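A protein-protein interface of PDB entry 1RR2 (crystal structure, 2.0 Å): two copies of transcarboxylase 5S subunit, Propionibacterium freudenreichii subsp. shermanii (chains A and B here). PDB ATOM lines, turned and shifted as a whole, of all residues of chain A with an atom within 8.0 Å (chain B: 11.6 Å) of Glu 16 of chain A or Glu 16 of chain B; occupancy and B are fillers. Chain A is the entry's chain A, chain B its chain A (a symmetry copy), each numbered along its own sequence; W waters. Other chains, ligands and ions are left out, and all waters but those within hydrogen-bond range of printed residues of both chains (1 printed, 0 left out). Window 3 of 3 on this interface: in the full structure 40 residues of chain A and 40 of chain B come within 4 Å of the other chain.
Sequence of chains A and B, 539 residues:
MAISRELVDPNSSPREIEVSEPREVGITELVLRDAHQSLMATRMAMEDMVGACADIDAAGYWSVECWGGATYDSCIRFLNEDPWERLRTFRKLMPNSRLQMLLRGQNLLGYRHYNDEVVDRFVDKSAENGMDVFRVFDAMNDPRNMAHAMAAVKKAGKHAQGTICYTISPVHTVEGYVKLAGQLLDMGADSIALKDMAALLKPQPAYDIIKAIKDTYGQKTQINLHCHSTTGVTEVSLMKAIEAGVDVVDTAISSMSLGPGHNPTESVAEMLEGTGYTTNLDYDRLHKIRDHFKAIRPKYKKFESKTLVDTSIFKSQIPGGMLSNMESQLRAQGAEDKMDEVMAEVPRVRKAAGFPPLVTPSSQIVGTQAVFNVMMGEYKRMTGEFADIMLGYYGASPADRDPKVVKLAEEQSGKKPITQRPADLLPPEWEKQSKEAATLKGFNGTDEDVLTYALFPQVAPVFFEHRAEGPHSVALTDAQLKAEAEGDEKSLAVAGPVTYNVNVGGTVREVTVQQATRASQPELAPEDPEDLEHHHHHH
The backbone carbonyl oxygen (O) of Arg 15 of chain A sits at hydrogen-bond distance from the backbone NH (N) of Val 19 of chain B, at 3.0 Å. NH1 of Arg 15 of chain A is in hydrogen-bond range of O of Ser 20 of chain B, at 2.8 Å. NH2 of Arg 15 of chain A is in hydrogen-bond range of O of Thr 275 of chain B, at 2.5 Å. NH1 of Arg 15 of chain A sits at hydrogen-bond distance from OH of Tyr 277 of chain B (3.2 Å). The side-chain carboxylate of Glu 16 of chain B lies close to the side-chain carboxylate of Glu 16 of chain A, at 2.6 Å. The backbone NH of Ile 17 of chain B lies within hydrogen-bond range of the backbone carbonyl oxygen of Ile 17 of chain A, 2.8 Å away. N of Val 19 of chain A sits at hydrogen-bond distance from O of Arg 15 of chain B (3.0 Å). O of Ser 20 of chain A is in hydrogen-bond range of NH1 of Arg 15 of chain B (2.8 Å).
The backbone carbonyl oxygen (O) of Glu 18 of chain A lies within hydrogen-bond range of the side-chain hydroxyl (OH) of Tyr 207 of chain A (2.6 Å). The backbone carbonyl oxygen (O) of Glu 18 of chain B sits at hydrogen-bond distance from the side-chain hydroxyl (OH) of Tyr 207 of chain B (2.6 Å). The backbone carbonyl oxygen of Ile 242 of chain B is in hydrogen-bond range of the side-chain hydroxyl of Ser 20 of chain B, at 2.8 Å. The backbone NH of Ser 20 of chain B lies within hydrogen-bond range of the backbone carbonyl oxygen of Glu 243 of chain B, 2.8 Å away. O of Ser 20 of chain B sits at hydrogen-bond distance from OH of Tyr 277 of chain B (2.8 Å). The side-chain hydroxyl (OG1) of Thr 275 of chain B lies within hydrogen-bond range of the backbone NH (N) of Tyr 277 of chain B (3.1 Å).
Among the printed residues, merely in contact across the chains: Ile 17 of chain A with Glu 16 of chain B, Glu 16 of chain A with Ile 17 of chain B, Arg 15 of chain A with Glu 18 of chain B, Glu 18 of chain A with Arg 15 of chain B, Arg 15 of chain A with Pro 22 of chain B, Arg 15 of chain A with Gly 276 of chain B, Ile 17 of chain A with Val 19 of chain B, Val 19 of chain A with Ile 17 of chain B, Glu 21 of chain A with Arg 15 of chain B and Arg 15 of chain A with Glu 21 of chain B.
No residue of chain B comes within 4 Å of Pro 14 of chain A. Arg 15 of chain A touches just these residues of chain B: Glu 18, Val 19, Ser 20, Glu 21, Pro 22, Thr 275, Gly 276 and Tyr 277. Glu 16 of chain A touches two residues of chain B. Glu 18 of chain A touches just one residue of chain B: Arg 15 (3.5 Å). Val 19 of chain A touches two residues of chain B. Of the printed residues of chain B, Ser 20 of chain A touches Arg 15 (2.8 Å). Pro 14 of chain B touches none of the printed residues of chain A. Of chain A, only Glu 16 (2.6 Å) and Ile 17 (3.3 Å) come within 4 Å of Glu 16 of chain B. Of the printed residues of chain A, Glu 18 of chain B touches Arg 15 (3.5 Å). Of the printed residues of chain A, Ser 20 of chain B touches Arg 15 (2.8 Å). Printed residues of chain A within 4 Å of Pro 22 of chain B: Arg 15. Gln 204 of chain B touches none of the printed residues of chain A. Of the printed residues of chain A, Tyr 277 of chain B touches Arg 15. The nearest residue of chain A that does not touch Glu 16 of chain B is Glu 18 of chain A (4.2 Å). The nearest printed residue of chain A that does not touch Thr 275 of chain B is Ile 17 of chain A (6.5 Å).
Of the 9 printed residues of chain A, 7 touch a printed residue of chain B. Hydrophobic or aromatic side chains of chain A that line the printed part of chain B: Ile 17 and Val 19. Among the printed residues, no Asp or Glu carboxylate lies within 4 Å of a Lys or Arg side-chain nitrogen of the other chain.
Arg 15 of chain A touches Glu 18 of chain B, and with the chains exchanged Glu 18 of chain A touches Arg 15 of chain B. Arg 15 of chain A touches Val 19 of chain B, and with the chains exchanged Val 19 of chain A touches Arg 15 of chain B. Arg 15 of chain A touches Glu 21 of chain B, and with the chains exchanged Glu 21 of chain A touches Arg 15 of chain B. Ile 17 of chain A touches its own counterpart, Ile 17 of chain B.
Water W1 bridges O of Thr 275 of chain B and NH2 of Arg 15 of chain A.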
ATOM      1  N   PRO A  14     -11.008 -13.272 -26.281  1.00  0.00           N
ATOM      2  CA  PRO A  14     -10.041 -12.175 -25.987  1.00  0.00           C
ATOM      3  C   PRO A  14      -8.620 -12.718 -26.165  1.00  0.00           C
ATOM      4  O   PRO A  14      -7.904 -13.013 -25.200  1.00  0.00           O
ATOM      5  CB  PRO A  14     -10.323 -11.734 -24.562  1.00  0.00           C
ATOM      6  CG  PRO A  14     -11.833 -12.031 -24.467  1.00  0.00           C
ATOM      7  CD  PRO A  14     -12.004 -13.378 -25.198  1.00  0.00           C
ATOM      8  N   ARG A  15      -8.228 -12.808 -27.434  1.00  0.00           N
ATOM      9  CA  ARG A  15      -6.946 -13.372 -27.880  1.00  0.00           C
ATOM     10  C   ARG A  15      -5.748 -12.580 -27.353  1.00  0.00           C
ATOM     11  O   ARG A  15      -5.674 -11.363 -27.501  1.00  0.00           O
ATOM     12  CB  ARG A  15      -6.968 -13.415 -29.398  1.00  0.00           C
ATOM     13  CG  ARG A  15      -5.856 -14.256 -30.024  1.00  0.00           C
ATOM     14  CD  ARG A  15      -6.114 -14.436 -31.522  1.00  0.00           C
ATOM     15  NE  ARG A  15      -5.275 -15.344 -32.285  1.00  0.00           N
ATOM     16  CZ  ARG A  15      -4.392 -14.967 -33.198  1.00  0.00           C
ATOM     17  NH1 ARG A  15      -4.230 -13.679 -33.485  1.00  0.00           N
ATOM     18  NH2 ARG A  15      -3.663 -15.892 -33.810  1.00  0.00           N
ATOM     19  N   GLU A  16      -4.795 -13.293 -26.760  1.00  0.00           N
ATOM     20  CA  GLU A  16      -3.603 -12.649 -26.192  1.00  0.00           C
ATOM     21  C   GLU A  16      -2.366 -13.484 -26.452  1.00  0.00           C
ATOM     22  O   GLU A  16      -2.447 -14.671 -26.763  1.00  0.00           O
ATOM     23  CB  GLU A  16      -3.759 -12.520 -24.697  1.00  0.00           C
ATOM     24  CG  GLU A  16      -5.075 -11.845 -24.313  1.00  0.00           C
ATOM     25  CD  GLU A  16      -5.015 -11.298 -22.933  1.00  0.00           C
ATOM     26  OE1 GLU A  16      -5.124 -10.059 -22.796  1.00  0.00           O
ATOM     27  OE2 GLU A  16      -4.844 -12.107 -21.995  1.00  0.00           O
ATOM     28  N   ILE A  17      -1.211 -12.850 -26.296  1.00  0.00           N
ATOM     29  CA  ILE A  17       0.077 -13.533 -26.475  1.00  0.00           C
ATOM     30  C   ILE A  17       0.949 -13.212 -25.275  1.00  0.00           C
ATOM     31  O   ILE A  17       1.144 -12.051 -24.931  1.00  0.00           O
ATOM     32  CB  ILE A  17       0.797 -13.058 -27.758  1.00  0.00           C
ATOM     33  CG1 ILE A  17       0.006 -13.506 -28.992  1.00  0.00           C
ATOM     34  CG2 ILE A  17       2.215 -13.626 -27.799  1.00  0.00           C
ATOM     35  CD1 ILE A  17       0.658 -13.106 -30.312  1.00  0.00           C
ATOM     36  N   GLU A  18       1.462 -14.238 -24.620  1.00  0.00           N
ATOM     37  CA  GLU A  18       2.324 -13.994 -23.457  1.00  0.00           C
ATOM     38  C   GLU A  18       3.704 -13.551 -23.944  1.00  0.00           C
ATOM     39  O   GLU A  18       4.275 -14.156 -24.855  1.00  0.00           O
ATOM     40  CB  GLU A  18       2.437 -15.263 -22.624  1.00  0.00           C
ATOM     41  CG  GLU A  18       3.378 -15.094 -21.431  1.00  0.00           C
ATOM     42  CD  GLU A  18       3.389 -16.303 -20.546  1.00  0.00           C
ATOM     43  OE1 GLU A  18       3.588 -17.421 -21.071  1.00  0.00           O
ATOM     44  OE2 GLU A  18       3.202 -16.125 -19.327  1.00  0.00           O
ATOM     45  N   VAL A  19       4.233 -12.482 -23.360  1.00  0.00           N
ATOM     46  CA  VAL A  19       5.566 -12.015 -23.763  1.00  0.00           C
ATOM     47  C   VAL A  19       6.459 -11.934 -22.533  1.00  0.00           C
ATOM     48  O   VAL A  19       5.965 -11.813 -21.413  1.00  0.00           O
ATOM     49  CB  VAL A  19       5.505 -10.649 -24.447  1.00  0.00           C
ATOM     50  CG1 VAL A  19       4.679 -10.763 -25.718  1.00  0.00           C
ATOM     51  CG2 VAL A  19       4.911  -9.617 -23.503  1.00  0.00           C
ATOM     52  N   SER A  20       7.768 -11.996 -22.746  1.00  0.00           N
ATOM     53  CA  SER A  20       8.729 -11.956 -21.635  1.00  0.00           C
ATOM     54  C   SER A  20       8.685 -10.587 -20.971  1.00  0.00           C
ATOM     55  O   SER A  20       8.299  -9.586 -21.577  1.00  0.00           O
ATOM     56  CB  SER A  20      10.142 -12.261 -22.144  1.00  0.00           C
ATOM     57  OG  SER A  20      10.506 -11.375 -23.192  1.00  0.00           O
ATOM     58  N   GLU A  21       9.082 -10.559 -19.709  1.00  0.00           N
ATOM     59  CA  GLU A  21       9.091  -9.326 -18.908  1.00  0.00           C
ATOM     60  C   GLU A  21      10.112  -8.345 -19.488  1.00  0.00           C
ATOM     61  O   GLU A  21      11.049  -8.746 -20.188  1.00  0.00           O
ATOM     62  CB  GLU A  21       9.473  -9.653 -17.462  1.00  0.00           C
ATOM     63  CG  GLU A  21      10.898 -10.185 -17.298  1.00  0.00           C
ATOM     64  CD  GLU A  21      11.140 -11.543 -17.964  1.00  0.00           C
ATOM     65  OE1 GLU A  21      12.324 -11.942 -18.059  1.00  0.00           O
ATOM     66  OE2 GLU A  21      10.165 -12.220 -18.382  1.00  0.00           O
ATOM     67  N   TYR A 207       9.056 -17.824 -32.102  1.00  0.00           N
ATOM     68  CA  TYR A 207       8.443 -17.677 -30.775  1.00  0.00           C
ATOM     69  C   TYR A 207       8.239 -19.063 -30.156  1.00  0.00           C
ATOM     70  O   TYR A 207       8.685 -19.315 -29.049  1.00  0.00           O
ATOM     71  CB  TYR A 207       7.092 -16.964 -30.902  1.00  0.00           C
ATOM     72  CG  TYR A 207       6.338 -16.826 -29.592  1.00  0.00           C
ATOM     73  CD1 TYR A 207       6.468 -15.685 -28.800  1.00  0.00           C
ATOM     74  CD2 TYR A 207       5.504 -17.846 -29.141  1.00  0.00           C
ATOM     75  CE1 TYR A 207       5.782 -15.569 -27.597  1.00  0.00           C
ATOM     76  CE2 TYR A 207       4.813 -17.739 -27.934  1.00  0.00           C
ATOM     77  CZ  TYR A 207       4.954 -16.604 -27.174  1.00  0.00           C
ATOM     78  OH  TYR A 207       4.243 -16.490 -26.002  1.00  0.00           O
ATOM     79  N   PRO B  14       2.453 -11.850 -15.105  1.00  0.00           N
ATOM     80  CA  PRO B  14       2.230 -12.670 -16.331  1.00  0.00           C
ATOM     81  C   PRO B  14       1.875 -11.730 -17.487  1.00  0.00           C
ATOM     82  O   PRO B  14       0.714 -11.601 -17.896  1.00  0.00           O
ATOM     83  CB  PRO B  14       1.106 -13.634 -15.996  1.00  0.00           C
ATOM     84  CG  PRO B  14       1.331 -13.815 -14.482  1.00  0.00           C
ATOM     85  CD  PRO B  14       1.681 -12.401 -13.975  1.00  0.00           C
ATOM     86  N   ARG B  15       2.923 -11.105 -18.020  1.00  0.00           N
ATOM     87  CA  ARG B  15       2.847 -10.092 -19.082  1.00  0.00           C
ATOM     88  C   ARG B  15       2.264 -10.656 -20.380  1.00  0.00           C
ATOM     89  O   ARG B  15       2.716 -11.677 -20.891  1.00  0.00           O
ATOM     90  CB  ARG B  15       4.245  -9.538 -19.288  1.00  0.00           C
ATOM     91  CG  ARG B  15       4.303  -8.261 -20.127  1.00  0.00           C
ATOM     92  CD  ARG B  15       5.707  -7.655 -20.064  1.00  0.00           C
ATOM     93  NE  ARG B  15       5.945  -6.347 -20.648  1.00  0.00           N
ATOM     94  CZ  ARG B  15       6.663  -6.128 -21.739  1.00  0.00           C
ATOM     95  NH1 ARG B  15       7.241  -7.140 -22.379  1.00  0.00           N
ATOM     96  NH2 ARG B  15       6.785  -4.886 -22.193  1.00  0.00           N
ATOM     97  N   GLU B  16       1.270  -9.957 -20.923  1.00  0.00           N
ATOM     98  CA  GLU B  16       0.611 -10.404 -22.158  1.00  0.00           C
ATOM     99  C   GLU B  16       0.299  -9.224 -23.056  1.00  0.00           C
ATOM    100  O   GLU B  16       0.282  -8.074 -22.622  1.00  0.00           O
ATOM    101  CB  GLU B  16      -0.696 -11.076 -21.821  1.00  0.00           C
ATOM    102  CG  GLU B  16      -0.523 -12.177 -20.775  1.00  0.00           C
ATOM    103  CD  GLU B  16      -1.665 -13.127 -20.800  1.00  0.00           C
ATOM    104  OE1 GLU B  16      -1.422 -14.316 -21.104  1.00  0.00           O
ATOM    105  OE2 GLU B  16      -2.800 -12.676 -20.531  1.00  0.00           O
ATOM    106  N   ILE B  17       0.029  -9.529 -24.318  1.00  0.00           N
ATOM    107  CA  ILE B  17      -0.330  -8.501 -25.304  1.00  0.00           C
ATOM    108  C   ILE B  17      -1.578  -8.962 -26.032  1.00  0.00           C
ATOM    109  O   ILE B  17      -1.629 -10.069 -26.557  1.00  0.00           O
ATOM    110  CB  ILE B  17       0.800  -8.287 -26.336  1.00  0.00           C
ATOM    111  CG1 ILE B  17       2.026  -7.678 -25.647  1.00  0.00           C
ATOM    112  CG2 ILE B  17       0.313  -7.373 -27.460  1.00  0.00           C
ATOM    113  CD1 ILE B  17       3.187  -7.403 -26.596  1.00  0.00           C
ATOM    114  N   GLU B  18      -2.601  -8.125 -26.049  1.00  0.00           N
ATOM    115  CA  GLU B  18      -3.836  -8.508 -26.747  1.00  0.00           C
ATOM    116  C   GLU B  18      -3.622  -8.358 -28.254  1.00  0.00           C
ATOM    117  O   GLU B  18      -3.095  -7.344 -28.717  1.00  0.00           O
ATOM    118  CB  GLU B  18      -4.984  -7.624 -26.282  1.00  0.00           C
ATOM    119  CG  GLU B  18      -6.287  -7.927 -27.022  1.00  0.00           C
ATOM    120  CD  GLU B  18      -7.442  -7.144 -26.476  1.00  0.00           C
ATOM    121  OE1 GLU B  18      -7.315  -5.905 -26.359  1.00  0.00           O
ATOM    122  OE2 GLU B  18      -8.471  -7.775 -26.171  1.00  0.00           O
ATOM    123  N   VAL B  19      -4.006  -9.373 -29.018  1.00  0.00           N
ATOM    124  CA  VAL B  19      -3.853  -9.287 -30.477  1.00  0.00           C
ATOM    125  C   VAL B  19      -5.201  -9.537 -31.136  1.00  0.00           C
ATOM    126  O   VAL B  19      -6.076 -10.168 -30.543  1.00  0.00           O
ATOM    127  CB  VAL B  19      -2.828 -10.294 -30.999  1.00  0.00           C
ATOM    128  CG1 VAL B  19      -1.468  -9.982 -30.396  1.00  0.00           C
ATOM    129  CG2 VAL B  19      -3.264 -11.709 -30.656  1.00  0.00           C
ATOM    130  N   SER B  20      -5.362  -9.049 -32.360  1.00  0.00           N
ATOM    131  CA  SER B  20      -6.631  -9.203 -33.086  1.00  0.00           C
ATOM    132  C   SER B  20      -6.857 -10.672 -33.412  1.00  0.00           C
ATOM    133  O   SER B  20      -5.920 -11.469 -33.496  1.00  0.00           O
ATOM    134  CB  SER B  20      -6.611  -8.365 -34.370  1.00  0.00           C
ATOM    135  OG  SER B  20      -5.493  -8.700 -35.178  1.00  0.00           O
ATOM    136  N   GLU B  21      -8.122 -11.023 -33.590  1.00  0.00           N
ATOM    137  CA  GLU B  21      -8.525 -12.403 -33.896  1.00  0.00           C
ATOM    138  C   GLU B  21      -7.985 -12.803 -35.270  1.00  0.00           C
ATOM    139  O   GLU B  21      -7.692 -11.945 -36.110  1.00  0.00           O
ATOM    140  CB  GLU B  21     -10.052 -12.502 -33.907  1.00  0.00           C
ATOM    141  CG  GLU B  21     -10.722 -11.689 -35.017  1.00  0.00           C
ATOM    142  CD  GLU B  21     -10.543 -10.174 -34.879  1.00  0.00           C
ATOM    143  OE1 GLU B  21     -10.873  -9.458 -35.852  1.00  0.00           O
ATOM    144  OE2 GLU B  21     -10.088  -9.691 -33.809  1.00  0.00           O
ATOM    145  N   PRO B  22      -7.842 -14.116 -35.513  1.00  0.00           N
ATOM    146  CA  PRO B  22      -7.343 -14.642 -36.788  1.00  0.00           C
ATOM    147  C   PRO B  22      -8.165 -14.003 -37.891  1.00  0.00           C
ATOM    148  O   PRO B  22      -9.375 -13.858 -37.767  1.00  0.00           O
ATOM    149  CB  PRO B  22      -7.593 -16.135 -36.659  1.00  0.00           C
ATOM    150  CG  PRO B  22      -7.329 -16.357 -35.160  1.00  0.00           C
ATOM    151  CD  PRO B  22      -8.091 -15.208 -34.547  1.00  0.00           C
ATOM    152  N   GLN B 204       5.966  -0.342 -31.356  1.00  0.00           N
ATOM    153  CA  GLN B 204       5.027  -0.053 -30.262  1.00  0.00           C
ATOM    154  C   GLN B 204       4.045   1.046 -30.666  1.00  0.00           C
ATOM    155  O   GLN B 204       2.837   0.921 -30.445  1.00  0.00           O
ATOM    156  CB  GLN B 204       5.768   0.327 -28.981  1.00  0.00           C
ATOM    157  CG  GLN B 204       4.831   0.284 -27.771  1.00  0.00           C
ATOM    158  CD  GLN B 204       4.255  -1.107 -27.569  1.00  0.00           C
ATOM    159  OE1 GLN B 204       5.000  -2.071 -27.393  1.00  0.00           O
ATOM    160  NE2 GLN B 204       2.927  -1.219 -27.591  1.00  0.00           N
ATOM    161  N   TYR B 207       1.356  -0.242 -33.028  1.00  0.00           N
ATOM    162  CA  TYR B 207       0.329  -0.999 -32.301  1.00  0.00           C
ATOM    163  C   TYR B 207      -0.572  -0.024 -31.537  1.00  0.00           C
ATOM    164  O   TYR B 207      -1.782  -0.057 -31.687  1.00  0.00           O
ATOM    165  CB  TYR B 207       0.995  -1.967 -31.316  1.00  0.00           C
ATOM    166  CG  TYR B 207       0.017  -2.749 -30.459  1.00  0.00           C
ATOM    167  CD1 TYR B 207      -0.436  -4.010 -30.846  1.00  0.00           C
ATOM    168  CD2 TYR B 207      -0.463  -2.219 -29.264  1.00  0.00           C
ATOM    169  CE1 TYR B 207      -1.339  -4.718 -30.061  1.00  0.00           C
ATOM    170  CE2 TYR B 207      -1.371  -2.920 -28.470  1.00  0.00           C
ATOM    171  CZ  TYR B 207      -1.798  -4.162 -28.871  1.00  0.00           C
ATOM    172  OH  TYR B 207      -2.667  -4.863 -28.067  1.00  0.00           O
ATOM    173  N   ASP B 208       0.027   0.872 -30.760  1.00  0.00           N
ATOM    174  CA  ASP B 208      -0.747   1.794 -29.914  1.00  0.00           C
ATOM    175  C   ASP B 208      -1.663   2.711 -30.724  1.00  0.00           C
ATOM    176  O   ASP B 208      -2.823   2.921 -30.348  1.00  0.00           O
ATOM    177  CB  ASP B 208       0.175   2.652 -29.062  1.00  0.00           C
ATOM    178  CG  ASP B 208       0.964   1.844 -28.047  1.00  0.00           C
ATOM    179  OD1 ASP B 208       0.690   0.634 -27.869  1.00  0.00           O
ATOM    180  OD2 ASP B 208       1.866   2.437 -27.415  1.00  0.00           O
ATOM    181  N   LYS B 211      -4.470   0.576 -32.537  1.00  0.00           N
ATOM    182  CA  LYS B 211      -5.382   0.066 -31.504  1.00  0.00           C
ATOM    183  C   LYS B 211      -6.259   1.204 -30.958  1.00  0.00           C
ATOM    184  O   LYS B 211      -7.453   1.021 -30.740  1.00  0.00           O
ATOM    185  CB  LYS B 211      -4.574  -0.544 -30.357  1.00  0.00           C
ATOM    186  CG  LYS B 211      -5.433  -1.307 -29.345  1.00  0.00           C
ATOM    187  CD  LYS B 211      -6.160  -2.459 -30.040  1.00  0.00           C
ATOM    188  CE  LYS B 211      -6.974  -3.288 -29.045  1.00  0.00           C
ATOM    189  NZ  LYS B 211      -6.090  -4.036 -28.114  1.00  0.00           N
ATOM    190  N   LYS B 240       3.189  -5.536 -35.885  1.00  0.00           N
ATOM    191  CA  LYS B 240       2.490  -4.980 -34.717  1.00  0.00           C
ATOM    192  C   LYS B 240       1.155  -4.391 -35.117  1.00  0.00           C
ATOM    193  O   LYS B 240       0.155  -4.559 -34.399  1.00  0.00           O
ATOM    194  CB  LYS B 240       3.352  -3.921 -34.026  1.00  0.00           C
ATOM    195  CG  LYS B 240       4.479  -4.564 -33.220  1.00  0.00           C
ATOM    196  CD  LYS B 240       3.873  -5.432 -32.115  1.00  0.00           C
ATOM    197  CE  LYS B 240       4.938  -6.267 -31.404  1.00  0.00           C
ATOM    198  NZ  LYS B 240       4.223  -7.101 -30.401  1.00  0.00           N
ATOM    199  N   ILE B 242      -0.719  -5.295 -37.510  1.00  0.00           N
ATOM    200  CA  ILE B 242      -1.663  -6.387 -37.781  1.00  0.00           C
ATOM    201  C   ILE B 242      -2.182  -6.942 -36.458  1.00  0.00           C
ATOM    202  O   ILE B 242      -3.366  -7.260 -36.335  1.00  0.00           O
ATOM    203  CB  ILE B 242      -1.002  -7.486 -38.624  1.00  0.00           C
ATOM    204  CG1 ILE B 242      -0.769  -6.951 -40.045  1.00  0.00           C
ATOM    205  CG2 ILE B 242      -1.879  -8.722 -38.664  1.00  0.00           C
ATOM    206  CD1 ILE B 242       0.102  -7.837 -40.925  1.00  0.00           C
ATOM    207  N   GLU B 243      -1.312  -7.050 -35.462  1.00  0.00           N
ATOM    208  CA  GLU B 243      -1.766  -7.541 -34.152  1.00  0.00           C
ATOM    209  C   GLU B 243      -2.756  -6.530 -33.563  1.00  0.00           C
ATOM    210  O   GLU B 243      -3.691  -6.908 -32.855  1.00  0.00           O
ATOM    211  CB  GLU B 243      -0.570  -7.743 -33.206  1.00  0.00           C
ATOM    212  CG  GLU B 243       0.441  -8.770 -33.714  1.00  0.00           C
ATOM    213  CD  GLU B 243       1.689  -8.862 -32.841  1.00  0.00           C
ATOM    214  OE1 GLU B 243       2.164  -7.808 -32.366  1.00  0.00           O
ATOM    215  OE2 GLU B 243       2.198  -9.988 -32.638  1.00  0.00           O
ATOM    216  N   ALA B 244      -2.563  -5.253 -33.882  1.00  0.00           N
ATOM    217  CA  ALA B 244      -3.435  -4.186 -33.369  1.00  0.00           C
ATOM    218  C   ALA B 244      -4.728  -4.133 -34.167  1.00  0.00           C
ATOM    219  O   ALA B 244      -5.637  -3.377 -33.819  1.00  0.00           O
ATOM    220  CB  ALA B 244      -2.731  -2.841 -33.436  1.00  0.00           C
ATOM    221  N   GLY B 274       1.183 -19.388 -39.739  1.00  0.00           N
ATOM    222  CA  GLY B 274       1.060 -19.916 -38.391  1.00  0.00           C
ATOM    223  C   GLY B 274       0.598 -18.928 -37.328  1.00  0.00           C
ATOM    224  O   GLY B 274       0.301 -19.327 -36.204  1.00  0.00           O
ATOM    225  N   THR B 275       0.512 -17.644 -37.664  1.00  0.00           N
ATOM    226  CA  THR B 275       0.123 -16.636 -36.667  1.00  0.00           C
ATOM    227  C   THR B 275      -1.402 -16.536 -36.527  1.00  0.00           C
ATOM    228  O   THR B 275      -1.892 -15.953 -35.565  1.00  0.00           O
ATOM    229  CB  THR B 275       0.645 -15.229 -37.046  1.00  0.00           C
ATOM    230  OG1 THR B 275      -0.001 -14.784 -38.250  1.00  0.00           O
ATOM    231  CG2 THR B 275       2.173 -15.252 -37.267  1.00  0.00           C
ATOM    232  N   GLY B 276      -2.150 -17.090 -37.473  1.00  0.00           N
ATOM    233  CA  GLY B 276      -3.597 -16.969 -37.428  1.00  0.00           C
ATOM    234  C   GLY B 276      -3.993 -15.905 -38.446  1.00  0.00           C
ATOM    235  O   GLY B 276      -5.149 -15.797 -38.869  1.00  0.00           O
ATOM    236  N   TYR B 277      -3.021 -15.095 -38.842  1.00  0.00           N
ATOM    237  CA  TYR B 277      -3.274 -14.057 -39.851  1.00  0.00           C
ATOM    238  C   TYR B 277      -2.834 -14.583 -41.196  1.00  0.00           C
ATOM    239  O   TYR B 277      -1.927 -15.413 -41.295  1.00  0.00           O
ATOM    240  CB  TYR B 277      -2.482 -12.800 -39.545  1.00  0.00           C
ATOM    241  CG  TYR B 277      -2.733 -12.271 -38.170  1.00  0.00           C
ATOM    242  CD1 TYR B 277      -1.707 -12.211 -37.228  1.00  0.00           C
ATOM    243  CD2 TYR B 277      -3.999 -11.824 -37.800  1.00  0.00           C
ATOM    244  CE1 TYR B 277      -1.941 -11.712 -35.946  1.00  0.00           C
ATOM    245  CE2 TYR B 277      -4.238 -11.320 -36.527  1.00  0.00           C
ATOM    246  CZ  TYR B 277      -3.203 -11.265 -35.613  1.00  0.00           C
ATOM    247  OH  TYR B 277      -3.422 -10.721 -34.380  1.00  0.00           O
HETATM  248  O   HOH W   1      -0.896 -14.213 -33.625  1.00  0.00           O
